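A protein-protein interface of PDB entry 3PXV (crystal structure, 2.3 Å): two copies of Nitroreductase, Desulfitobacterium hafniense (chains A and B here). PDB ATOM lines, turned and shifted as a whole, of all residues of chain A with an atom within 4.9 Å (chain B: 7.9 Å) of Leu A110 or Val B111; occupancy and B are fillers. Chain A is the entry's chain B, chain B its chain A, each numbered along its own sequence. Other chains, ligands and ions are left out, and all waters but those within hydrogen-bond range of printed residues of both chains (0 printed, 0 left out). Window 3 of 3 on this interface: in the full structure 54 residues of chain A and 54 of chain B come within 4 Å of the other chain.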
ATOM      1  N   ILE A 101       2.511 -15.341   4.798  1.00  0.00           N
ATOM      2  CA  ILE A 101       3.375 -14.603   5.701  1.00  0.00           C
ATOM      3  C   ILE A 101       4.741 -14.362   5.079  1.00  0.00           C
ATOM      4  O   ILE A 101       5.137 -15.054   4.129  1.00  0.00           O
ATOM      5  CB  ILE A 101       3.532 -15.325   7.085  1.00  0.00           C
ATOM      6  CG1 ILE A 101       4.179 -16.696   6.951  1.00  0.00           C
ATOM      7  CG2 ILE A 101       2.209 -15.503   7.810  1.00  0.00           C
ATOM      8  CD1 ILE A 101       4.633 -17.226   8.315  1.00  0.00           C
ATOM      9  N   TYR A 106      10.896 -14.742  10.165  1.00  0.00           N
ATOM     10  CA  TYR A 106      11.102 -15.971  10.941  1.00  0.00           C
ATOM     11  C   TYR A 106       9.998 -16.299  11.982  1.00  0.00           C
ATOM     12  O   TYR A 106       8.817 -16.228  11.662  1.00  0.00           O
ATOM     13  CB  TYR A 106      12.531 -15.934  11.544  1.00  0.00           C
ATOM     14  CG  TYR A 106      13.610 -15.660  10.490  1.00  0.00           C
ATOM     15  CD1 TYR A 106      14.062 -16.678   9.635  1.00  0.00           C
ATOM     16  CD2 TYR A 106      14.144 -14.379  10.322  1.00  0.00           C
ATOM     17  CE1 TYR A 106      15.017 -16.428   8.650  1.00  0.00           C
ATOM     18  CE2 TYR A 106      15.105 -14.119   9.340  1.00  0.00           C
ATOM     19  CZ  TYR A 106      15.538 -15.147   8.507  1.00  0.00           C
ATOM     20  OH  TYR A 106      16.496 -14.891   7.543  1.00  0.00           O
ATOM     21  N   GLY A 107      10.388 -16.661  13.204  1.00  0.00           N
ATOM     22  CA  GLY A 107       9.452 -17.032  14.260  1.00  0.00           C
ATOM     23  C   GLY A 107       8.448 -15.973  14.627  1.00  0.00           C
ATOM     24  O   GLY A 107       7.286 -16.274  14.872  1.00  0.00           O
ATOM     25  N   PRO A 108       8.889 -14.723  14.702  1.00  0.00           N
ATOM     26  CA  PRO A 108       7.899 -13.708  15.039  1.00  0.00           C
ATOM     27  C   PRO A 108       6.698 -13.655  14.067  1.00  0.00           C
ATOM     28  O   PRO A 108       5.598 -13.358  14.492  1.00  0.00           O
ATOM     29  CB  PRO A 108       8.726 -12.401  15.044  1.00  0.00           C
ATOM     30  CG  PRO A 108      10.095 -12.833  15.451  1.00  0.00           C
ATOM     31  CD  PRO A 108      10.268 -14.229  14.878  1.00  0.00           C
ATOM     32  N   ALA A 109       6.916 -13.945  12.784  1.00  0.00           N
ATOM     33  CA  ALA A 109       5.814 -13.944  11.805  1.00  0.00           C
ATOM     34  C   ALA A 109       4.814 -15.106  12.016  1.00  0.00           C
ATOM     35  O   ALA A 109       3.642 -14.981  11.707  1.00  0.00           O
ATOM     36  CB  ALA A 109       6.363 -13.963  10.409  1.00  0.00           C
ATOM     37  N   LEU A 110       5.292 -16.230  12.535  1.00  0.00           N
ATOM     38  CA  LEU A 110       4.429 -17.351  12.837  1.00  0.00           C
ATOM     39  C   LEU A 110       3.557 -17.049  14.050  1.00  0.00           C
ATOM     40  O   LEU A 110       2.385 -17.313  14.000  1.00  0.00           O
ATOM     41  CB  LEU A 110       5.236 -18.638  13.018  1.00  0.00           C
ATOM     42  CG  LEU A 110       5.757 -19.206  11.682  1.00  0.00           C
ATOM     43  CD1 LEU A 110       6.813 -20.250  11.951  1.00  0.00           C
ATOM     44  CD2 LEU A 110       4.650 -19.797  10.849  1.00  0.00           C
ATOM     45  N   VAL A 111       4.115 -16.515  15.131  1.00  0.00           N
ATOM     46  CA  VAL A 111       3.323 -16.118  16.306  1.00  0.00           C
ATOM     47  C   VAL A 111       2.179 -15.173  15.823  1.00  0.00           C
ATOM     48  O   VAL A 111       0.975 -15.471  15.991  1.00  0.00           O
ATOM     49  CB  VAL A 111       4.230 -15.445  17.371  1.00  0.00           C
ATOM     50  CG1 VAL A 111       3.403 -14.758  18.458  1.00  0.00           C
ATOM     51  CG2 VAL A 111       5.279 -16.473  17.973  1.00  0.00           C
ATOM     52  N   ASP A 112       2.556 -14.097  15.131  1.00  0.00           N
ATOM     53  CA  ASP A 112       1.599 -13.158  14.574  1.00  0.00           C
ATOM     54  C   ASP A 112       0.556 -13.875  13.738  1.00  0.00           C
ATOM     55  O   ASP A 112      -0.638 -13.529  13.782  1.00  0.00           O
ATOM     56  CB  ASP A 112       2.288 -12.100  13.695  1.00  0.00           C
ATOM     57  CG  ASP A 112       3.201 -11.164  14.485  1.00  0.00           C
ATOM     58  OD1 ASP A 112       3.078 -11.069  15.721  1.00  0.00           O
ATOM     59  OD2 ASP A 112       4.050 -10.503  13.873  1.00  0.00           O
ATOM     60  N   CYS A 113       1.002 -14.871  12.972  1.00  0.00           N
ATOM     61  CA  CYS A 113       0.107 -15.625  12.124  1.00  0.00           C
ATOM     62  C   CYS A 113      -0.970 -16.313  12.941  1.00  0.00           C
ATOM     63  O   CYS A 113      -2.156 -16.262  12.566  1.00  0.00           O
ATOM     64  CB  CYS A 113       0.861 -16.649  11.258  1.00  0.00           C
ATOM     65  SG  CYS A 113      -0.244 -17.662  10.193  1.00  0.00           S
ATOM     66  N   GLY A 114      -0.563 -16.945  14.048  1.00  0.00           N
ATOM     67  CA  GLY A 114      -1.490 -17.647  14.938  1.00  0.00           C
ATOM     68  C   GLY A 114      -2.433 -16.688  15.638  1.00  0.00           C
ATOM     69  O   GLY A 114      -3.589 -16.994  15.859  1.00  0.00           O
ATOM     70  N   PRO B  40      -7.189 -23.482  20.444  1.00  0.00           N
ATOM     71  CA  PRO B  40      -6.917 -24.667  19.639  1.00  0.00           C
ATOM     72  C   PRO B  40      -5.407 -24.697  19.323  1.00  0.00           C
ATOM     73  O   PRO B  40      -4.717 -23.674  19.473  1.00  0.00           O
ATOM     74  CB  PRO B  40      -7.741 -24.423  18.377  1.00  0.00           C
ATOM     75  CG  PRO B  40      -7.836 -22.950  18.258  1.00  0.00           C
ATOM     76  CD  PRO B  40      -7.794 -22.395  19.660  1.00  0.00           C
ATOM     77  N   SER B  41      -4.921 -25.868  18.925  1.00  0.00           N
ATOM     78  CA  SER B  41      -3.522 -26.091  18.600  1.00  0.00           C
ATOM     79  C   SER B  41      -3.434 -27.221  17.576  1.00  0.00           C
ATOM     80  O   SER B  41      -4.274 -28.118  17.562  1.00  0.00           O
ATOM     81  CB  SER B  41      -2.727 -26.469  19.856  1.00  0.00           C
ATOM     82  OG  SER B  41      -3.218 -27.638  20.519  1.00  0.00           O
ATOM     83  N   GLY B  42      -2.436 -27.157  16.697  1.00  0.00           N
ATOM     84  CA  GLY B  42      -2.236 -28.172  15.688  1.00  0.00           C
ATOM     85  C   GLY B  42      -2.246 -29.532  16.350  1.00  0.00           C
ATOM     86  O   GLY B  42      -1.639 -29.732  17.413  1.00  0.00           O
ATOM     87  N   ARG B  45      -1.948 -30.644  20.034  1.00  0.00           N
ATOM     88  CA  ARG B  45      -0.663 -30.966  20.710  1.00  0.00           C
ATOM     89  C   ARG B  45      -0.458 -30.207  22.029  1.00  0.00           C
ATOM     90  O   ARG B  45       0.186 -30.700  22.936  1.00  0.00           O
ATOM     91  CB  ARG B  45       0.533 -30.723  19.793  1.00  0.00           C
ATOM     92  CG  ARG B  45       0.765 -29.250  19.390  1.00  0.00           C
ATOM     93  CD  ARG B  45       1.973 -29.083  18.472  1.00  0.00           C
ATOM     94  NE  ARG B  45       1.798 -29.641  17.133  1.00  0.00           N
ATOM     95  CZ  ARG B  45       1.363 -28.969  16.064  1.00  0.00           C
ATOM     96  NH1 ARG B  45       1.012 -27.684  16.133  1.00  0.00           N
ATOM     97  NH2 ARG B  45       1.256 -29.589  14.900  1.00  0.00           N
ATOM     98  N   TRP B  48       2.311 -26.173  25.068  1.00  0.00           N
ATOM     99  CA  TRP B  48       2.396 -24.976  25.828  1.00  0.00           C
ATOM    100  C   TRP B  48       1.884 -25.180  27.254  1.00  0.00           C
ATOM    101  O   TRP B  48       1.339 -26.229  27.577  1.00  0.00           O
ATOM    102  CB  TRP B  48       1.653 -23.810  25.125  1.00  0.00           C
ATOM    103  CG  TRP B  48       0.272 -24.097  24.497  1.00  0.00           C
ATOM    104  CD1 TRP B  48      -0.047 -23.982  23.184  1.00  0.00           C
ATOM    105  CD2 TRP B  48      -0.926 -24.535  25.155  1.00  0.00           C
ATOM    106  NE1 TRP B  48      -1.358 -24.296  22.981  1.00  0.00           N
ATOM    107  CE2 TRP B  48      -1.926 -24.630  24.172  1.00  0.00           C
ATOM    108  CE3 TRP B  48      -1.265 -24.815  26.489  1.00  0.00           C
ATOM    109  CZ2 TRP B  48      -3.233 -25.013  24.466  1.00  0.00           C
ATOM    110  CZ3 TRP B  48      -2.559 -25.201  26.775  1.00  0.00           C
ATOM    111  CH2 TRP B  48      -3.527 -25.290  25.770  1.00  0.00           C
ATOM    112  N   ILE B 101       6.856 -22.835  25.570  1.00  0.00           N
ATOM    113  CA  ILE B 101       6.519 -23.782  24.517  1.00  0.00           C
ATOM    114  C   ILE B 101       7.605 -24.844  24.365  1.00  0.00           C
ATOM    115  O   ILE B 101       8.717 -24.720  24.894  1.00  0.00           O
ATOM    116  CB  ILE B 101       6.267 -23.115  23.128  1.00  0.00           C
ATOM    117  CG1 ILE B 101       7.555 -22.491  22.567  1.00  0.00           C
ATOM    118  CG2 ILE B 101       5.086 -22.084  23.207  1.00  0.00           C
ATOM    119  CD1 ILE B 101       7.407 -21.837  21.165  1.00  0.00           C
ATOM    120  N   GLN B 105       9.092 -28.732  18.561  1.00  0.00           N
ATOM    121  CA  GLN B 105       7.962 -28.694  17.627  1.00  0.00           C
ATOM    122  C   GLN B 105       7.911 -27.317  16.928  1.00  0.00           C
ATOM    123  O   GLN B 105       6.859 -26.854  16.484  1.00  0.00           O
ATOM    124  CB  GLN B 105       6.644 -29.011  18.333  1.00  0.00           C
ATOM    125  CG  GLN B 105       6.680 -30.294  19.154  1.00  0.00           C
ATOM    126  CD  GLN B 105       5.309 -30.925  19.341  1.00  0.00           C
ATOM    127  OE1 GLN B 105       4.621 -31.227  18.375  1.00  0.00           O
ATOM    128  NE2 GLN B 105       4.929 -31.154  20.581  1.00  0.00           N
ATOM    129  N   TYR B 106       9.076 -26.678  16.891  1.00  0.00           N
ATOM    130  CA  TYR B 106       9.387 -25.435  16.175  1.00  0.00           C
ATOM    131  C   TYR B 106       8.236 -24.493  15.747  1.00  0.00           C
ATOM    132  O   TYR B 106       7.589 -23.871  16.583  1.00  0.00           O
ATOM    133  CB  TYR B 106      10.278 -25.804  14.949  1.00  0.00           C
ATOM    134  CG  TYR B 106      11.536 -26.622  15.304  1.00  0.00           C
ATOM    135  CD1 TYR B 106      12.707 -25.987  15.776  1.00  0.00           C
ATOM    136  CD2 TYR B 106      11.544 -28.024  15.194  1.00  0.00           C
ATOM    137  CE1 TYR B 106      13.855 -26.731  16.123  1.00  0.00           C
ATOM    138  CE2 TYR B 106      12.683 -28.775  15.535  1.00  0.00           C
ATOM    139  CZ  TYR B 106      13.832 -28.123  15.998  1.00  0.00           C
ATOM    140  OH  TYR B 106      14.946 -28.857  16.337  1.00  0.00           O
ATOM    141  N   GLY B 107       8.009 -24.394  14.439  1.00  0.00           N
ATOM    142  CA  GLY B 107       7.051 -23.472  13.845  1.00  0.00           C
ATOM    143  C   GLY B 107       5.631 -23.687  14.269  1.00  0.00           C
ATOM    144  O   GLY B 107       4.952 -22.749  14.614  1.00  0.00           O
ATOM    145  N   PRO B 108       5.171 -24.931  14.241  1.00  0.00           N
ATOM    146  CA  PRO B 108       3.784 -25.117  14.639  1.00  0.00           C
ATOM    147  C   PRO B 108       3.517 -24.719  16.094  1.00  0.00           C
ATOM    148  O   PRO B 108       2.455 -24.200  16.376  1.00  0.00           O
ATOM    149  CB  PRO B 108       3.537 -26.588  14.370  1.00  0.00           C
ATOM    150  CG  PRO B 108       4.524 -26.947  13.241  1.00  0.00           C
ATOM    151  CD  PRO B 108       5.712 -26.071  13.476  1.00  0.00           C
ATOM    152  N   ALA B 109       4.457 -24.947  16.995  1.00  0.00           N
ATOM    153  CA  ALA B 109       4.306 -24.527  18.395  1.00  0.00           C
ATOM    154  C   ALA B 109       4.273 -22.991  18.502  1.00  0.00           C
ATOM    155  O   ALA B 109       3.541 -22.457  19.327  1.00  0.00           O
ATOM    156  CB  ALA B 109       5.401 -25.111  19.263  1.00  0.00           C
ATOM    157  N   LEU B 110       5.028 -22.286  17.656  1.00  0.00           N
ATOM    158  CA  LEU B 110       5.013 -20.810  17.647  1.00  0.00           C
ATOM    159  C   LEU B 110       3.657 -20.305  17.160  1.00  0.00           C
ATOM    160  O   LEU B 110       3.114 -19.345  17.713  1.00  0.00           O
ATOM    161  CB  LEU B 110       6.135 -20.215  16.794  1.00  0.00           C
ATOM    162  CG  LEU B 110       7.564 -20.241  17.346  1.00  0.00           C
ATOM    163  CD1 LEU B 110       8.545 -19.868  16.249  1.00  0.00           C
ATOM    164  CD2 LEU B 110       7.762 -19.340  18.572  1.00  0.00           C
ATOM    165  N   VAL B 111       3.105 -20.951  16.141  1.00  0.00           N
ATOM    166  CA  VAL B 111       1.767 -20.591  15.666  1.00  0.00           C
ATOM    167  C   VAL B 111       0.731 -20.833  16.776  1.00  0.00           C
ATOM    168  O   VAL B 111      -0.139 -19.983  17.018  1.00  0.00           O
ATOM    169  CB  VAL B 111       1.326 -21.396  14.425  1.00  0.00           C
ATOM    170  CG1 VAL B 111      -0.116 -21.018  14.063  1.00  0.00           C
ATOM    171  CG2 VAL B 111       2.295 -21.189  13.267  1.00  0.00           C
ATOM    172  N   ASP B 112       0.827 -21.981  17.452  1.00  0.00           N
ATOM    173  CA  ASP B 112      -0.074 -22.277  18.569  1.00  0.00           C
ATOM    174  C   ASP B 112       0.129 -21.275  19.718  1.00  0.00           C
ATOM    175  O   ASP B 112      -0.826 -20.933  20.416  1.00  0.00           O
ATOM    176  CB  ASP B 112       0.118 -23.694  19.114  1.00  0.00           C
ATOM    177  CG  ASP B 112      -0.127 -24.800  18.070  1.00  0.00           C
ATOM    178  OD1 ASP B 112      -0.807 -24.547  17.047  1.00  0.00           O
ATOM    179  OD2 ASP B 112       0.373 -25.944  18.305  1.00  0.00           O
ATOM    180  N   CYS B 113       1.361 -20.817  19.927  1.00  0.00           N
ATOM    181  CA  CYS B 113       1.645 -19.833  20.960  1.00  0.00           C
ATOM    182  C   CYS B 113       0.850 -18.545  20.710  1.00  0.00           C
ATOM    183  O   CYS B 113       0.215 -18.020  21.610  1.00  0.00           O
ATOM    184  CB  CYS B 113       3.123 -19.506  20.978  1.00  0.00           C
ATOM    185  SG  CYS B 113       3.625 -18.481  22.342  1.00  0.00           S
ATOM    186  N   GLY B 114       0.885 -18.062  19.472  1.00  0.00           N
ATOM    187  CA  GLY B 114       0.159 -16.860  19.067  1.00  0.00           C
ATOM    188  C   GLY B 114      -1.341 -17.017  19.243  1.00  0.00           C
ATOM    189  O   GLY B 114      -2.018 -16.125  19.731  1.00  0.00           O
ATOM    190  N   ILE B 115      -1.861 -18.187  18.893  1.00  0.00           N
ATOM    191  CA  ILE B 115      -3.284 -18.457  19.043  1.00  0.00           C
ATOM    192  C   ILE B 115      -3.693 -18.294  20.494  1.00  0.00           C
ATOM    193  O   ILE B 115      -4.682 -17.663  20.793  1.00  0.00           O
ATOM    194  CB  ILE B 115      -3.608 -19.856  18.563  1.00  0.00           C
ATOM    195  CG1 ILE B 115      -3.545 -19.926  17.030  1.00  0.00           C
ATOM    196  CG2 ILE B 115      -4.998 -20.305  19.059  1.00  0.00           C
ATOM    197  CD1 ILE B 115      -3.695 -21.381  16.463  1.00  0.00           C
ATOM    198  N   LEU B 116      -2.900 -18.852  21.386  1.00  0.00           N
ATOM    199  CA  LEU B 116      -3.173 -18.845  22.809  1.00  0.00           C
ATOM    200  C   LEU B 116      -3.024 -17.448  23.418  1.00  0.00           C
ATOM    201  O   LEU B 116      -3.905 -16.998  24.178  1.00  0.00           O
ATOM    202  CB  LEU B 116      -2.287 -19.906  23.527  1.00  0.00           C
ATOM    203  CG  LEU B 116      -2.418 -20.107  25.041  1.00  0.00           C
ATOM    204  CD1 LEU B 116      -2.174 -21.586  25.474  1.00  0.00           C
ATOM    205  CD2 LEU B 116      -1.543 -19.117  25.784  1.00  0.00           C
ATOM    206  N   CYS B 117      -1.935 -16.746  23.094  1.00  0.00           N
ATOM    207  CA  CYS B 117      -1.751 -15.374  23.627  1.00  0.00           C
ATOM    208  C   CYS B 117      -2.884 -14.451  23.177  1.00  0.00           C
ATOM    209  O   CYS B 117      -3.295 -13.588  23.946  1.00  0.00           O
ATOM    210  CB  CYS B 117      -0.364 -14.782  23.273  1.00  0.00           C
ATOM    211  SG  CYS B 117       0.968 -15.686  24.068  1.00  0.00           S
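Printed residues of chain A that touch a printed residue of chain B: Gly A107, Leu A110, Val A111 and Gly A114.
Hydrophobic or aromatic side chains of chain A that line the printed part of chain B: Leu A110 and Val A111.
Among the printed residues, 8 pairs touch across the chains.
Among the printed residues, no Asp or Glu carboxylate lies within 4 Å of a Lys or Arg side-chain nitrogen of the other chain.
Gly A107 touches Leu B110, and with the chains exchanged Leu A110 touches Gly B107.
Leu A110 touches Val B111, and with the chains exchanged Val A111 touches Leu B110.
Val A111 touches Gly B114, and with the chains exchanged Gly A114 touches Val B111.
Gly B114 touches its own counterpart, Gly A114.
Of the 8 pairs that touch across the chains among the printed residues, 7 have their exchanged pair printed and touching as well.
CA of Gly A107 touches CD1 of Leu B110, 3.6 Å away.
Leu A110 touches Gly B107.
CD2 of Leu A110 touches CG2 of Val B111 (3.7 Å).
Leu B110 touches Val A111 (O to CA, 3.5 Å).
Val A111 touches Gly B114.
Gly A114 touches Val B111 (CA to O, 3.4 Å).
Gly A114 touches Gly B114.
O of Gly A114 touches CG1 of Ile B115 (3.2 Å).
Printed residues of chain B within 4 Å of Gly A107: Leu B110.
Ala A109 touches none of the printed residues of chain B.
Leu A110 touches just these residues of chain B: Gly B107 and Val B111.
Printed residues of chain B within 4 Å of Val A111: Leu B110 (3.5 Å) and Gly B114 (3.5 Å).
Of the printed residues of chain B, Gly A114 touches Val B111, Gly B114 and Ile B115.
Gln B105 touches none of the printed residues of chain A.
Pro B108 touches none of the printed residues of chain A.
Of chain A, only Leu A110 and Gly A114 come within 4 Å of Val B111.
Of the printed residues of chain A, Gly B114 touches Val A111 and Gly A114.
The nearest residue of chain B that does not touch Leu A110 is Leu B110 (4.2 Å).
The nearest residue of chain A that does not touch Val B111 is Val A111 (4.7 Å).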
